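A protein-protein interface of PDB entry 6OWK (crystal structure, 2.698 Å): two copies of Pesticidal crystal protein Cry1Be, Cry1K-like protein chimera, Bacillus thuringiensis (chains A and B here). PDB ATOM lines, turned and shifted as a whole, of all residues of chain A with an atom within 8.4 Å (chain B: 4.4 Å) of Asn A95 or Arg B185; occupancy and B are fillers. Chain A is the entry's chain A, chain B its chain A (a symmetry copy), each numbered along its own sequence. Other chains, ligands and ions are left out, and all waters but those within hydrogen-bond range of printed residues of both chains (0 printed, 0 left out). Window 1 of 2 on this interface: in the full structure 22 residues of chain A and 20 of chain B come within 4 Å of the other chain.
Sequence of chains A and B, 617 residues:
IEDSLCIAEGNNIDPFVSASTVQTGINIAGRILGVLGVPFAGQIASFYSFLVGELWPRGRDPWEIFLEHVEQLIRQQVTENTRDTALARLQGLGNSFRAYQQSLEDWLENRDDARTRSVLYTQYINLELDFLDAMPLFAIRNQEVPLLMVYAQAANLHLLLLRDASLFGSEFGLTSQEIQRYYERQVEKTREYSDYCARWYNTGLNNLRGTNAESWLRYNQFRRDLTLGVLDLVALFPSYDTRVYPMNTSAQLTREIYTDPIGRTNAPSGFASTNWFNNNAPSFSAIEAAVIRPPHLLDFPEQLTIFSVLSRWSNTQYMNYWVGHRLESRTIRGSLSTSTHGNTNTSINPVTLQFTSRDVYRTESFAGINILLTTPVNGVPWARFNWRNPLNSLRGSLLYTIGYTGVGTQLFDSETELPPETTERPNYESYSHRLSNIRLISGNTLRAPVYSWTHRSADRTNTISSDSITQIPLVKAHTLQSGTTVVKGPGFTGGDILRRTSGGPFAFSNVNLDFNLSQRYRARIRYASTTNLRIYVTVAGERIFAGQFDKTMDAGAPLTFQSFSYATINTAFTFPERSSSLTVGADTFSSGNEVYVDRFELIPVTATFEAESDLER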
ATOM      1  N   VAL A  52       2.688 -12.090   7.906  1.00  0.00           N
ATOM      2  CA  VAL A  52       1.702 -11.047   7.646  1.00  0.00           C
ATOM      3  C   VAL A  52       1.790  -9.952   8.688  1.00  0.00           C
ATOM      4  O   VAL A  52       1.470  -8.793   8.406  1.00  0.00           O
ATOM      5  CB  VAL A  52       0.274 -11.603   7.601  1.00  0.00           C
ATOM      6  CG1 VAL A  52       0.113 -12.483   6.413  1.00  0.00           C
ATOM      7  CG2 VAL A  52      -0.069 -12.300   8.911  1.00  0.00           C
ATOM      8  N   TRP A  56       2.297  -7.047   6.502  1.00  0.00           N
ATOM      9  CA  TRP A  56       1.052  -6.289   6.457  1.00  0.00           C
ATOM     10  C   TRP A  56       0.578  -6.007   7.873  1.00  0.00           C
ATOM     11  O   TRP A  56      -0.326  -6.681   8.383  1.00  0.00           O
ATOM     12  CB  TRP A  56      -0.013  -7.030   5.656  1.00  0.00           C
ATOM     13  CG  TRP A  56       0.355  -7.104   4.227  1.00  0.00           C
ATOM     14  CD1 TRP A  56       0.161  -6.144   3.279  1.00  0.00           C
ATOM     15  CD2 TRP A  56       1.027  -8.184   3.577  1.00  0.00           C
ATOM     16  NE1 TRP A  56       0.656  -6.567   2.070  1.00  0.00           N
ATOM     17  CE2 TRP A  56       1.198  -7.816   2.229  1.00  0.00           C
ATOM     18  CE3 TRP A  56       1.496  -9.429   4.003  1.00  0.00           C
ATOM     19  CZ2 TRP A  56       1.809  -8.653   1.302  1.00  0.00           C
ATOM     20  CZ3 TRP A  56       2.106 -10.255   3.083  1.00  0.00           C
ATOM     21  CH2 TRP A  56       2.256  -9.866   1.748  1.00  0.00           C
ATOM     22  N   ARG A  58      -0.862  -3.448  11.123  1.00  0.00           N
ATOM     23  CA  ARG A  58      -1.748  -2.315  11.290  1.00  0.00           C
ATOM     24  C   ARG A  58      -0.919  -1.041  11.416  1.00  0.00           C
ATOM     25  O   ARG A  58       0.255  -1.068  11.795  1.00  0.00           O
ATOM     26  CB  ARG A  58      -2.641  -2.503  12.516  1.00  0.00           C
ATOM     27  CG  ARG A  58      -3.649  -3.634  12.377  1.00  0.00           C
ATOM     28  CD  ARG A  58      -4.773  -3.255  11.427  1.00  0.00           C
ATOM     29  NE  ARG A  58      -5.508  -4.420  10.943  1.00  0.00           N
ATOM     30  CZ  ARG A  58      -5.422  -4.898   9.706  1.00  0.00           C
ATOM     31  NH1 ARG A  58      -4.630  -4.311   8.818  1.00  0.00           N
ATOM     32  NH2 ARG A  58      -6.129  -5.964   9.355  1.00  0.00           N
ATOM     33  N   LEU A  87       2.091  -0.343  -4.795  1.00  0.00           N
ATOM     34  CA  LEU A  87       1.546  -0.449  -3.445  1.00  0.00           C
ATOM     35  C   LEU A  87       0.088  -0.880  -3.464  1.00  0.00           C
ATOM     36  O   LEU A  87      -0.363  -1.604  -2.569  1.00  0.00           O
ATOM     37  CB  LEU A  87       1.699   0.881  -2.710  1.00  0.00           C
ATOM     38  CG  LEU A  87       3.130   1.381  -2.565  1.00  0.00           C
ATOM     39  CD1 LEU A  87       3.092   2.751  -1.953  1.00  0.00           C
ATOM     40  CD2 LEU A  87       3.952   0.427  -1.714  1.00  0.00           C
ATOM     41  N   ALA A  88      -0.670  -0.419  -4.459  1.00  0.00           N
ATOM     42  CA  ALA A  88      -2.039  -0.890  -4.617  1.00  0.00           C
ATOM     43  C   ALA A  88      -2.063  -2.388  -4.896  1.00  0.00           C
ATOM     44  O   ALA A  88      -2.851  -3.133  -4.302  1.00  0.00           O
ATOM     45  CB  ALA A  88      -2.734  -0.117  -5.735  1.00  0.00           C
ATOM     46  N   ARG A  89      -1.196  -2.847  -5.800  1.00  0.00           N
ATOM     47  CA  ARG A  89      -1.068  -4.280  -6.038  1.00  0.00           C
ATOM     48  C   ARG A  89      -0.605  -5.010  -4.781  1.00  0.00           C
ATOM     49  O   ARG A  89      -1.017  -6.149  -4.529  1.00  0.00           O
ATOM     50  CB  ARG A  89      -0.097  -4.533  -7.193  1.00  0.00           C
ATOM     51  CG  ARG A  89       0.109  -6.003  -7.527  1.00  0.00           C
ATOM     52  CD  ARG A  89      -1.068  -6.562  -8.305  1.00  0.00           C
ATOM     53  NE  ARG A  89      -1.903  -7.437  -7.486  1.00  0.00           N
ATOM     54  CZ  ARG A  89      -2.502  -8.531  -7.941  1.00  0.00           C
ATOM     55  NH1 ARG A  89      -2.360  -8.889  -9.210  1.00  0.00           N
ATOM     56  NH2 ARG A  89      -3.246  -9.269  -7.128  1.00  0.00           N
ATOM     57  N   LEU A  90       0.228  -4.359  -3.963  1.00  0.00           N
ATOM     58  CA  LEU A  90       0.845  -5.049  -2.834  1.00  0.00           C
ATOM     59  C   LEU A  90      -0.158  -5.330  -1.719  1.00  0.00           C
ATOM     60  O   LEU A  90      -0.197  -6.446  -1.183  1.00  0.00           O
ATOM     61  CB  LEU A  90       2.025  -4.232  -2.305  1.00  0.00           C
ATOM     62  CG  LEU A  90       3.369  -4.636  -2.914  1.00  0.00           C
ATOM     63  CD1 LEU A  90       4.433  -3.594  -2.619  1.00  0.00           C
ATOM     64  CD2 LEU A  90       3.792  -6.013  -2.411  1.00  0.00           C
ATOM     65  N   GLN A  91      -0.969  -4.328  -1.348  1.00  0.00           N
ATOM     66  CA  GLN A  91      -1.943  -4.492  -0.265  1.00  0.00           C
ATOM     67  C   GLN A  91      -3.056  -5.445  -0.644  1.00  0.00           C
ATOM     68  O   GLN A  91      -3.498  -6.250   0.189  1.00  0.00           O
ATOM     69  CB  GLN A  91      -2.525  -3.134   0.150  1.00  0.00           C
ATOM     70  CG  GLN A  91      -1.499  -2.049   0.271  1.00  0.00           C
ATOM     71  CD  GLN A  91      -2.087  -0.655   0.245  1.00  0.00           C
ATOM     72  OE1 GLN A  91      -3.108  -0.373   0.877  1.00  0.00           O
ATOM     73  NE2 GLN A  91      -1.426   0.239  -0.479  1.00  0.00           N
ATOM     74  N   GLY A  92      -3.551  -5.332  -1.874  1.00  0.00           N
ATOM     75  CA  GLY A  92      -4.497  -6.312  -2.354  1.00  0.00           C
ATOM     76  C   GLY A  92      -3.940  -7.720  -2.289  1.00  0.00           C
ATOM     77  O   GLY A  92      -4.625  -8.655  -1.863  1.00  0.00           O
ATOM     78  N   LEU A  93      -2.688  -7.890  -2.717  1.00  0.00           N
ATOM     79  CA  LEU A  93      -1.991  -9.156  -2.523  1.00  0.00           C
ATOM     80  C   LEU A  93      -1.889  -9.522  -1.048  1.00  0.00           C
ATOM     81  O   LEU A  93      -1.892 -10.708  -0.698  1.00  0.00           O
ATOM     82  CB  LEU A  93      -0.600  -9.063  -3.150  1.00  0.00           C
ATOM     83  CG  LEU A  93       0.344 -10.258  -3.125  1.00  0.00           C
ATOM     84  CD1 LEU A  93      -0.337 -11.484  -3.703  1.00  0.00           C
ATOM     85  CD2 LEU A  93       1.568  -9.882  -3.929  1.00  0.00           C
ATOM     86  N   GLY A  94      -1.790  -8.519  -0.172  1.00  0.00           N
ATOM     87  CA  GLY A  94      -1.752  -8.786   1.253  1.00  0.00           C
ATOM     88  C   GLY A  94      -3.098  -9.145   1.837  1.00  0.00           C
ATOM     89  O   GLY A  94      -3.173  -9.951   2.769  1.00  0.00           O
ATOM     90  N   ASN A  95      -4.175  -8.548   1.318  1.00  0.00           N
ATOM     91  CA  ASN A  95      -5.511  -9.010   1.676  1.00  0.00           C
ATOM     92  C   ASN A  95      -5.691 -10.471   1.293  1.00  0.00           C
ATOM     93  O   ASN A  95      -6.323 -11.244   2.023  1.00  0.00           O
ATOM     94  CB  ASN A  95      -6.566  -8.146   0.990  1.00  0.00           C
ATOM     95  CG  ASN A  95      -6.563  -6.713   1.482  1.00  0.00           C
ATOM     96  OD1 ASN A  95      -6.532  -6.454   2.687  1.00  0.00           O
ATOM     97  ND2 ASN A  95      -6.593  -5.769   0.546  1.00  0.00           N
ATOM     98  N   SER A  96      -5.128 -10.867   0.152  1.00  0.00           N
ATOM     99  CA  SER A  96      -5.207 -12.249  -0.299  1.00  0.00           C
ATOM    100  C   SER A  96      -4.260 -13.144   0.487  1.00  0.00           C
ATOM    101  O   SER A  96      -4.615 -14.273   0.841  1.00  0.00           O
ATOM    102  CB  SER A  96      -4.882 -12.316  -1.789  1.00  0.00           C
ATOM    103  OG  SER A  96      -5.384 -11.169  -2.452  1.00  0.00           O
ATOM    104  N   PHE A  97      -3.043 -12.659   0.748  1.00  0.00           N
ATOM    105  CA  PHE A  97      -2.100 -13.429   1.552  1.00  0.00           C
ATOM    106  C   PHE A  97      -2.620 -13.613   2.970  1.00  0.00           C
ATOM    107  O   PHE A  97      -2.468 -14.689   3.562  1.00  0.00           O
ATOM    108  CB  PHE A  97      -0.735 -12.739   1.554  1.00  0.00           C
ATOM    109  CG  PHE A  97       0.381 -13.601   2.065  1.00  0.00           C
ATOM    110  CD1 PHE A  97       1.073 -14.448   1.216  1.00  0.00           C
ATOM    111  CD2 PHE A  97       0.740 -13.559   3.394  1.00  0.00           C
ATOM    112  CE1 PHE A  97       2.101 -15.237   1.695  1.00  0.00           C
ATOM    113  CE2 PHE A  97       1.763 -14.343   3.881  1.00  0.00           C
ATOM    114  CZ  PHE A  97       2.445 -15.182   3.031  1.00  0.00           C
ATOM    115  N   ARG A  98      -3.251 -12.576   3.526  1.00  0.00           N
ATOM    116  CA  ARG A  98      -3.880 -12.710   4.835  1.00  0.00           C
ATOM    117  C   ARG A  98      -5.030 -13.708   4.788  1.00  0.00           C
ATOM    118  O   ARG A  98      -5.244 -14.465   5.741  1.00  0.00           O
ATOM    119  CB  ARG A  98      -4.369 -11.347   5.321  1.00  0.00           C
ATOM    120  CG  ARG A  98      -4.943 -11.342   6.725  1.00  0.00           C
ATOM    121  CD  ARG A  98      -5.375  -9.940   7.128  1.00  0.00           C
ATOM    122  NE  ARG A  98      -5.336  -9.011   6.001  1.00  0.00           N
ATOM    123  CZ  ARG A  98      -4.886  -7.762   6.077  1.00  0.00           C
ATOM    124  NH1 ARG A  98      -4.433  -7.289   7.229  1.00  0.00           N
ATOM    125  NH2 ARG A  98      -4.889  -6.986   5.000  1.00  0.00           N
ATOM    126  N   ALA A  99      -5.777 -13.732   3.681  1.00  0.00           N
ATOM    127  CA  ALA A  99      -6.884 -14.675   3.555  1.00  0.00           C
ATOM    128  C   ALA A  99      -6.372 -16.104   3.429  1.00  0.00           C
ATOM    129  O   ALA A  99      -6.844 -17.006   4.131  1.00  0.00           O
ATOM    130  CB  ALA A  99      -7.756 -14.307   2.354  1.00  0.00           C
ATOM    131  N   TYR A 100      -5.404 -16.327   2.535  1.00  0.00           N
ATOM    132  CA  TYR A 100      -4.848 -17.666   2.356  1.00  0.00           C
ATOM    133  C   TYR A 100      -4.285 -18.211   3.662  1.00  0.00           C
ATOM    134  O   TYR A 100      -4.632 -19.319   4.083  1.00  0.00           O
ATOM    135  CB  TYR A 100      -3.771 -17.652   1.273  1.00  0.00           C
ATOM    136  CG  TYR A 100      -2.852 -18.853   1.317  1.00  0.00           C
ATOM    137  CD1 TYR A 100      -3.267 -20.092   0.844  1.00  0.00           C
ATOM    138  CD2 TYR A 100      -1.569 -18.748   1.837  1.00  0.00           C
ATOM    139  CE1 TYR A 100      -2.428 -21.190   0.884  1.00  0.00           C
ATOM    140  CE2 TYR A 100      -0.729 -19.840   1.888  1.00  0.00           C
ATOM    141  CZ  TYR A 100      -1.159 -21.057   1.406  1.00  0.00           C
ATOM    142  OH  TYR A 100      -0.320 -22.145   1.449  1.00  0.00           O
ATOM    143  N   GLN A 101      -3.411 -17.448   4.323  1.00  0.00           N
ATOM    144  CA  GLN A 101      -2.850 -17.926   5.581  1.00  0.00           C
ATOM    145  C   GLN A 101      -3.940 -18.134   6.627  1.00  0.00           C
ATOM    146  O   GLN A 101      -3.900 -19.108   7.385  1.00  0.00           O
ATOM    147  CB  GLN A 101      -1.805 -16.952   6.102  1.00  0.00           C
ATOM    148  CG  GLN A 101      -1.558 -17.070   7.599  1.00  0.00           C
ATOM    149  CD  GLN A 101      -1.612 -15.720   8.257  1.00  0.00           C
ATOM    150  OE1 GLN A 101      -1.163 -14.761   7.681  1.00  0.00           O
ATOM    151  NE2 GLN A 101      -2.161 -15.636   9.451  1.00  0.00           N
ATOM    152  N   GLN A 102      -4.921 -17.226   6.686  1.00  0.00           N
ATOM    153  CA  GLN A 102      -6.045 -17.391   7.607  1.00  0.00           C
ATOM    154  C   GLN A 102      -6.651 -18.780   7.481  1.00  0.00           C
ATOM    155  O   GLN A 102      -6.847 -19.480   8.478  1.00  0.00           O
ATOM    156  CB  GLN A 102      -7.110 -16.326   7.336  1.00  0.00           C
ATOM    157  CG  GLN A 102      -7.364 -15.365   8.481  1.00  0.00           C
ATOM    158  CD  GLN A 102      -8.367 -14.292   8.108  1.00  0.00           C
ATOM    159  OE1 GLN A 102      -8.461 -13.896   6.947  1.00  0.00           O
ATOM    160  NE2 GLN A 102      -9.130 -13.822   9.088  1.00  0.00           N
ATOM    161  N   SER A 103      -6.944 -19.201   6.250  1.00  0.00           N
ATOM    162  CA  SER A 103      -7.515 -20.525   6.040  1.00  0.00           C
ATOM    163  C   SER A 103      -6.448 -21.608   6.090  1.00  0.00           C
ATOM    164  O   SER A 103      -6.726 -22.731   6.526  1.00  0.00           O
ATOM    165  CB  SER A 103      -8.258 -20.571   4.712  1.00  0.00           C
ATOM    166  OG  SER A 103      -7.388 -20.954   3.661  1.00  0.00           O
ATOM    167  N   GLN A 123      -8.055 -20.416  -3.226  1.00  0.00           N
ATOM    168  CA  GLN A 123      -7.343 -19.211  -2.812  1.00  0.00           C
ATOM    169  C   GLN A 123      -5.832 -19.410  -2.850  1.00  0.00           C
ATOM    170  O   GLN A 123      -5.093 -18.443  -3.067  1.00  0.00           O
ATOM    171  CB  GLN A 123      -7.786 -18.762  -1.423  1.00  0.00           C
ATOM    172  CG  GLN A 123      -7.823 -19.853  -0.397  1.00  0.00           C
ATOM    173  CD  GLN A 123      -8.662 -19.484   0.799  1.00  0.00           C
ATOM    174  OE1 GLN A 123      -8.683 -20.200   1.792  1.00  0.00           O
ATOM    175  NE2 GLN A 123      -9.355 -18.355   0.714  1.00  0.00           N
ATOM    176  N   LEU A 127      -3.748 -17.097  -5.552  1.00  0.00           N
ATOM    177  CA  LEU A 127      -2.684 -16.229  -5.071  1.00  0.00           C
ATOM    178  C   LEU A 127      -1.349 -16.584  -5.713  1.00  0.00           C
ATOM    179  O   LEU A 127      -0.562 -15.692  -6.050  1.00  0.00           O
ATOM    180  CB  LEU A 127      -2.602 -16.315  -3.555  1.00  0.00           C
ATOM    181  CG  LEU A 127      -1.661 -15.332  -2.889  1.00  0.00           C
ATOM    182  CD1 LEU A 127      -2.300 -14.869  -1.638  1.00  0.00           C
ATOM    183  CD2 LEU A 127      -0.424 -16.078  -2.566  1.00  0.00           C
ATOM    184  N   LEU B 132     -10.760  -7.338  -3.418  1.00  0.00           N
ATOM    185  CA  LEU B 132      -9.717  -7.032  -2.444  1.00  0.00           C
ATOM    186  C   LEU B 132      -8.591  -6.227  -3.083  1.00  0.00           C
ATOM    187  O   LEU B 132      -8.253  -5.131  -2.622  1.00  0.00           O
ATOM    188  CB  LEU B 132      -9.175  -8.325  -1.833  1.00  0.00           C
ATOM    189  CG  LEU B 132     -10.060  -9.029  -0.805  1.00  0.00           C
ATOM    190  CD1 LEU B 132      -9.559 -10.442  -0.535  1.00  0.00           C
ATOM    191  CD2 LEU B 132     -10.129  -8.227   0.485  1.00  0.00           C
ATOM    192  N   LEU B 162     -19.837 -10.356   0.116  1.00  0.00           N
ATOM    193  CA  LEU B 162     -19.519 -11.007   1.378  1.00  0.00           C
ATOM    194  C   LEU B 162     -20.784 -11.376   2.137  1.00  0.00           C
ATOM    195  O   LEU B 162     -20.821 -12.407   2.820  1.00  0.00           O
ATOM    196  CB  LEU B 162     -18.624 -10.102   2.215  1.00  0.00           C
ATOM    197  CG  LEU B 162     -17.193 -10.032   1.680  1.00  0.00           C
ATOM    198  CD1 LEU B 162     -16.369  -8.996   2.427  1.00  0.00           C
ATOM    199  CD2 LEU B 162     -16.536 -11.403   1.753  1.00  0.00           C
ATOM    200  N   ARG B 181     -14.678 -17.125   8.067  1.00  0.00           N
ATOM    201  CA  ARG B 181     -13.575 -16.346   7.511  1.00  0.00           C
ATOM    202  C   ARG B 181     -14.088 -15.290   6.542  1.00  0.00           C
ATOM    203  O   ARG B 181     -13.557 -14.175   6.481  1.00  0.00           O
ATOM    204  CB  ARG B 181     -12.577 -17.269   6.809  1.00  0.00           C
ATOM    205  CG  ARG B 181     -11.895 -18.288   7.712  1.00  0.00           C
ATOM    206  CD  ARG B 181     -11.695 -17.760   9.123  1.00  0.00           C
ATOM    207  NE  ARG B 181     -10.520 -18.344   9.761  1.00  0.00           N
ATOM    208  CZ  ARG B 181      -9.623 -17.646  10.448  1.00  0.00           C
ATOM    209  NH1 ARG B 181      -9.766 -16.337  10.587  1.00  0.00           N
ATOM    210  NH2 ARG B 181      -8.582 -18.258  10.999  1.00  0.00           N
ATOM    211  N   TYR B 182     -15.134 -15.623   5.782  1.00  0.00           N
ATOM    212  CA  TYR B 182     -15.754 -14.639   4.902  1.00  0.00           C
ATOM    213  C   TYR B 182     -16.479 -13.564   5.699  1.00  0.00           C
ATOM    214  O   TYR B 182     -16.409 -12.377   5.359  1.00  0.00           O
ATOM    215  CB  TYR B 182     -16.715 -15.330   3.940  1.00  0.00           C
ATOM    216  CG  TYR B 182     -16.041 -15.778   2.674  1.00  0.00           C
ATOM    217  CD1 TYR B 182     -15.405 -14.862   1.850  1.00  0.00           C
ATOM    218  CD2 TYR B 182     -16.023 -17.115   2.305  1.00  0.00           C
ATOM    219  CE1 TYR B 182     -14.779 -15.262   0.695  1.00  0.00           C
ATOM    220  CE2 TYR B 182     -15.396 -17.525   1.148  1.00  0.00           C
ATOM    221  CZ  TYR B 182     -14.775 -16.592   0.346  1.00  0.00           C
ATOM    222  OH  TYR B 182     -14.148 -16.985  -0.810  1.00  0.00           O
ATOM    223  N   TYR B 183     -17.188 -13.961   6.758  1.00  0.00           N
ATOM    224  CA  TYR B 183     -17.908 -12.991   7.573  1.00  0.00           C
ATOM    225  C   TYR B 183     -16.960 -12.052   8.301  1.00  0.00           C
ATOM    226  O   TYR B 183     -17.296 -10.883   8.531  1.00  0.00           O
ATOM    227  CB  TYR B 183     -18.797 -13.717   8.580  1.00  0.00           C
ATOM    228  CG  TYR B 183     -19.482 -12.806   9.572  1.00  0.00           C
ATOM    229  CD1 TYR B 183     -20.717 -12.248   9.283  1.00  0.00           C
ATOM    230  CD2 TYR B 183     -18.906 -12.522  10.807  1.00  0.00           C
ATOM    231  CE1 TYR B 183     -21.348 -11.417  10.178  1.00  0.00           C
ATOM    232  CE2 TYR B 183     -19.538 -11.708  11.718  1.00  0.00           C
ATOM    233  CZ  TYR B 183     -20.758 -11.153  11.396  1.00  0.00           C
ATOM    234  OH  TYR B 183     -21.400 -10.330  12.291  1.00  0.00           O
ATOM    235  N   GLU B 184     -15.778 -12.541   8.679  1.00  0.00           N
ATOM    236  CA  GLU B 184     -14.859 -11.711   9.447  1.00  0.00           C
ATOM    237  C   GLU B 184     -14.349 -10.541   8.615  1.00  0.00           C
ATOM    238  O   GLU B 184     -14.254  -9.412   9.115  1.00  0.00           O
ATOM    239  CB  GLU B 184     -13.695 -12.555   9.962  1.00  0.00           C
ATOM    240  CG  GLU B 184     -14.101 -13.587  10.992  1.00  0.00           C
ATOM    241  CD  GLU B 184     -12.909 -14.158  11.725  1.00  0.00           C
ATOM    242  OE1 GLU B 184     -11.812 -13.564  11.631  1.00  0.00           O
ATOM    243  OE2 GLU B 184     -13.067 -15.199  12.392  1.00  0.00           O
ATOM    244  N   ARG B 185     -14.022 -10.800   7.340  1.00  0.00           N
ATOM    245  CA  ARG B 185     -13.599  -9.742   6.428  1.00  0.00           C
ATOM    246  C   ARG B 185     -14.744  -8.796   6.114  1.00  0.00           C
ATOM    247  O   ARG B 185     -14.516  -7.599   5.924  1.00  0.00           O
ATOM    248  CB  ARG B 185     -13.014 -10.362   5.144  1.00  0.00           C
ATOM    249  CG  ARG B 185     -11.831  -9.583   4.620  1.00  0.00           C
ATOM    250  CD  ARG B 185     -10.783  -9.363   5.734  1.00  0.00           C
ATOM    251  NE  ARG B 185      -9.963 -10.528   6.049  1.00  0.00           N
ATOM    252  CZ  ARG B 185      -8.893 -10.907   5.358  1.00  0.00           C
ATOM    253  NH1 ARG B 185      -8.533 -10.233   4.284  1.00  0.00           N
ATOM    254  NH2 ARG B 185      -8.201 -11.980   5.717  1.00  0.00           N
ATOM    255  N   GLN B 186     -15.969  -9.316   6.047  1.00  0.00           N
ATOM    256  CA  GLN B 186     -17.123  -8.436   5.908  1.00  0.00           C
ATOM    257  C   GLN B 186     -17.220  -7.481   7.089  1.00  0.00           C
ATOM    258  O   GLN B 186     -17.545  -6.299   6.922  1.00  0.00           O
ATOM    259  CB  GLN B 186     -18.422  -9.239   5.779  1.00  0.00           C
ATOM    260  CG  GLN B 186     -19.642  -8.348   5.568  1.00  0.00           C
ATOM    261  CD  GLN B 186     -20.965  -9.107   5.524  1.00  0.00           C
ATOM    262  OE1 GLN B 186     -20.997 -10.337   5.585  1.00  0.00           O
ATOM    263  NE2 GLN B 186     -22.065  -8.368   5.418  1.00  0.00           N
ATOM    264  N   VAL B 187     -16.947  -7.981   8.296  1.00  0.00           N
ATOM    265  CA  VAL B 187     -16.961  -7.123   9.476  1.00  0.00           C
ATOM    266  C   VAL B 187     -15.886  -6.051   9.363  1.00  0.00           C
ATOM    267  O   VAL B 187     -16.162  -4.853   9.503  1.00  0.00           O
ATOM    268  CB  VAL B 187     -16.789  -7.956  10.758  1.00  0.00           C
ATOM    269  CG1 VAL B 187     -16.586  -7.045  11.954  1.00  0.00           C
ATOM    270  CG2 VAL B 187     -18.001  -8.827  10.966  1.00  0.00           C
ATOM    271  N   GLU B 188     -14.642  -6.464   9.098  1.00  0.00           N
ATOM    272  CA  GLU B 188     -13.548  -5.495   9.070  1.00  0.00           C
ATOM    273  C   GLU B 188     -13.622  -4.606   7.837  1.00  0.00           C
ATOM    274  O   GLU B 188     -13.212  -3.440   7.889  1.00  0.00           O
ATOM    275  CB  GLU B 188     -12.186  -6.199   9.161  1.00  0.00           C
ATOM    276  CG  GLU B 188     -11.772  -6.992   7.944  1.00  0.00           C
ATOM    277  CD  GLU B 188     -10.280  -6.872   7.662  1.00  0.00           C
ATOM    278  OE1 GLU B 188      -9.566  -7.886   7.843  1.00  0.00           O
ATOM    279  OE2 GLU B 188      -9.834  -5.783   7.240  1.00  0.00           O
ATOM    280  N   LYS B 189     -14.136  -5.129   6.723  1.00  0.00           N
ATOM    281  CA  LYS B 189     -14.327  -4.274   5.558  1.00  0.00           C
ATOM    282  C   LYS B 189     -15.456  -3.280   5.783  1.00  0.00           C
ATOM    283  O   LYS B 189     -15.388  -2.147   5.294  1.00  0.00           O
ATOM    284  CB  LYS B 189     -14.596  -5.103   4.300  1.00  0.00           C
ATOM    285  CG  LYS B 189     -13.365  -5.792   3.727  1.00  0.00           C
ATOM    286  CD  LYS B 189     -12.124  -4.927   3.876  1.00  0.00           C
ATOM    287  CE  LYS B 189     -10.877  -5.656   3.406  1.00  0.00           C
ATOM    288  NZ  LYS B 189      -9.675  -4.779   3.463  1.00  0.00           N
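No position is printed for both chains. Of the 9 pairs that touch across the chains among the printed residues, none has its exchanged pair printed and touching as well.
The guanidinium group (NH1) of Arg B185 sits at hydrogen-bond distance from the backbone carbonyl oxygen (O) of Asn A95 (3.3 Å). NE2 of Gln A102 lies close to NH1 of Arg B181 (3.0 Å). The side-chain amide oxygen (OE1) of Gln A102 lies close to the guanidinium group (NH2) of Arg B185 (2.3 Å).
Among the printed residues, pairs that only touch across the chains: Gly A92 with Leu B132, Asn A95 with Leu B132, Asn A95 with Lys B189, Arg A98 with Arg B185, Ala A99 with Arg B185 and Gln A102 with Glu B184.
The side-chain amide nitrogen (ND2) of Asn A95 lies within hydrogen-bond range of the backbone carbonyl oxygen (O) of Gln A91 (3.2 Å). The side-chain hydroxyl (OG) of Ser A96 sits at hydrogen-bond distance from the backbone carbonyl oxygen (O) of Gly A92, at 2.7 Å. The guanidinium group (NH2) of Arg A98 is in hydrogen-bond range of the side-chain amide oxygen (OD1) of Asn A95 (2.9 Å). The side-chain amide oxygen of Gln A102 sits close to the backbone carbonyl oxygen of Arg A98. NH1 of Arg B181 lies within salt-bridge range of OE1 of Glu B184. The side-chain carboxylate of Glu B188 lies within salt-bridge range of the guanidinium group of Arg B185, at 3.2 Å.
Along chain A the printed residues that touch a printed residue of chain B span positions 92 to 102. Printed residues of chain B that touch a printed residue of chain A: Leu B132, Arg B181, Glu B184, Arg B185 and Lys B189. Among the printed residues, no Asp or Glu carboxylate lies within 4 Å of a Lys or Arg side-chain nitrogen of the other chain.
Gly A94 touches none of the printed residues of chain B. Asn A95 touches three residues of chain B. Of the printed residues of chain B, Arg A98 touches Arg B185 (3.5 Å). Printed residues of chain B within 4 Å of Gln A102: Arg B181 (3.0 Å), Glu B184 (3.7 Å) and Arg B185 (2.3 Å). Of the printed residues of chain A, Leu B132 touches Gly A92 (3.9 Å) and Asn A95 (3.6 Å). Of the printed residues of chain A, Arg B181 touches Gln A102. Printed residues of chain A within 4 Å of Glu B184: Gln A102. Of chain A, only Asn A95 (3.3 Å), Arg A98 (3.5 Å), Ala A99 (3.6 Å) and Gln A102 (2.3 Å) come within 4 Å of Arg B185. The nearest printed residue of chain A that does not touch Lys B189 is Arg A98 (5.5 Å).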
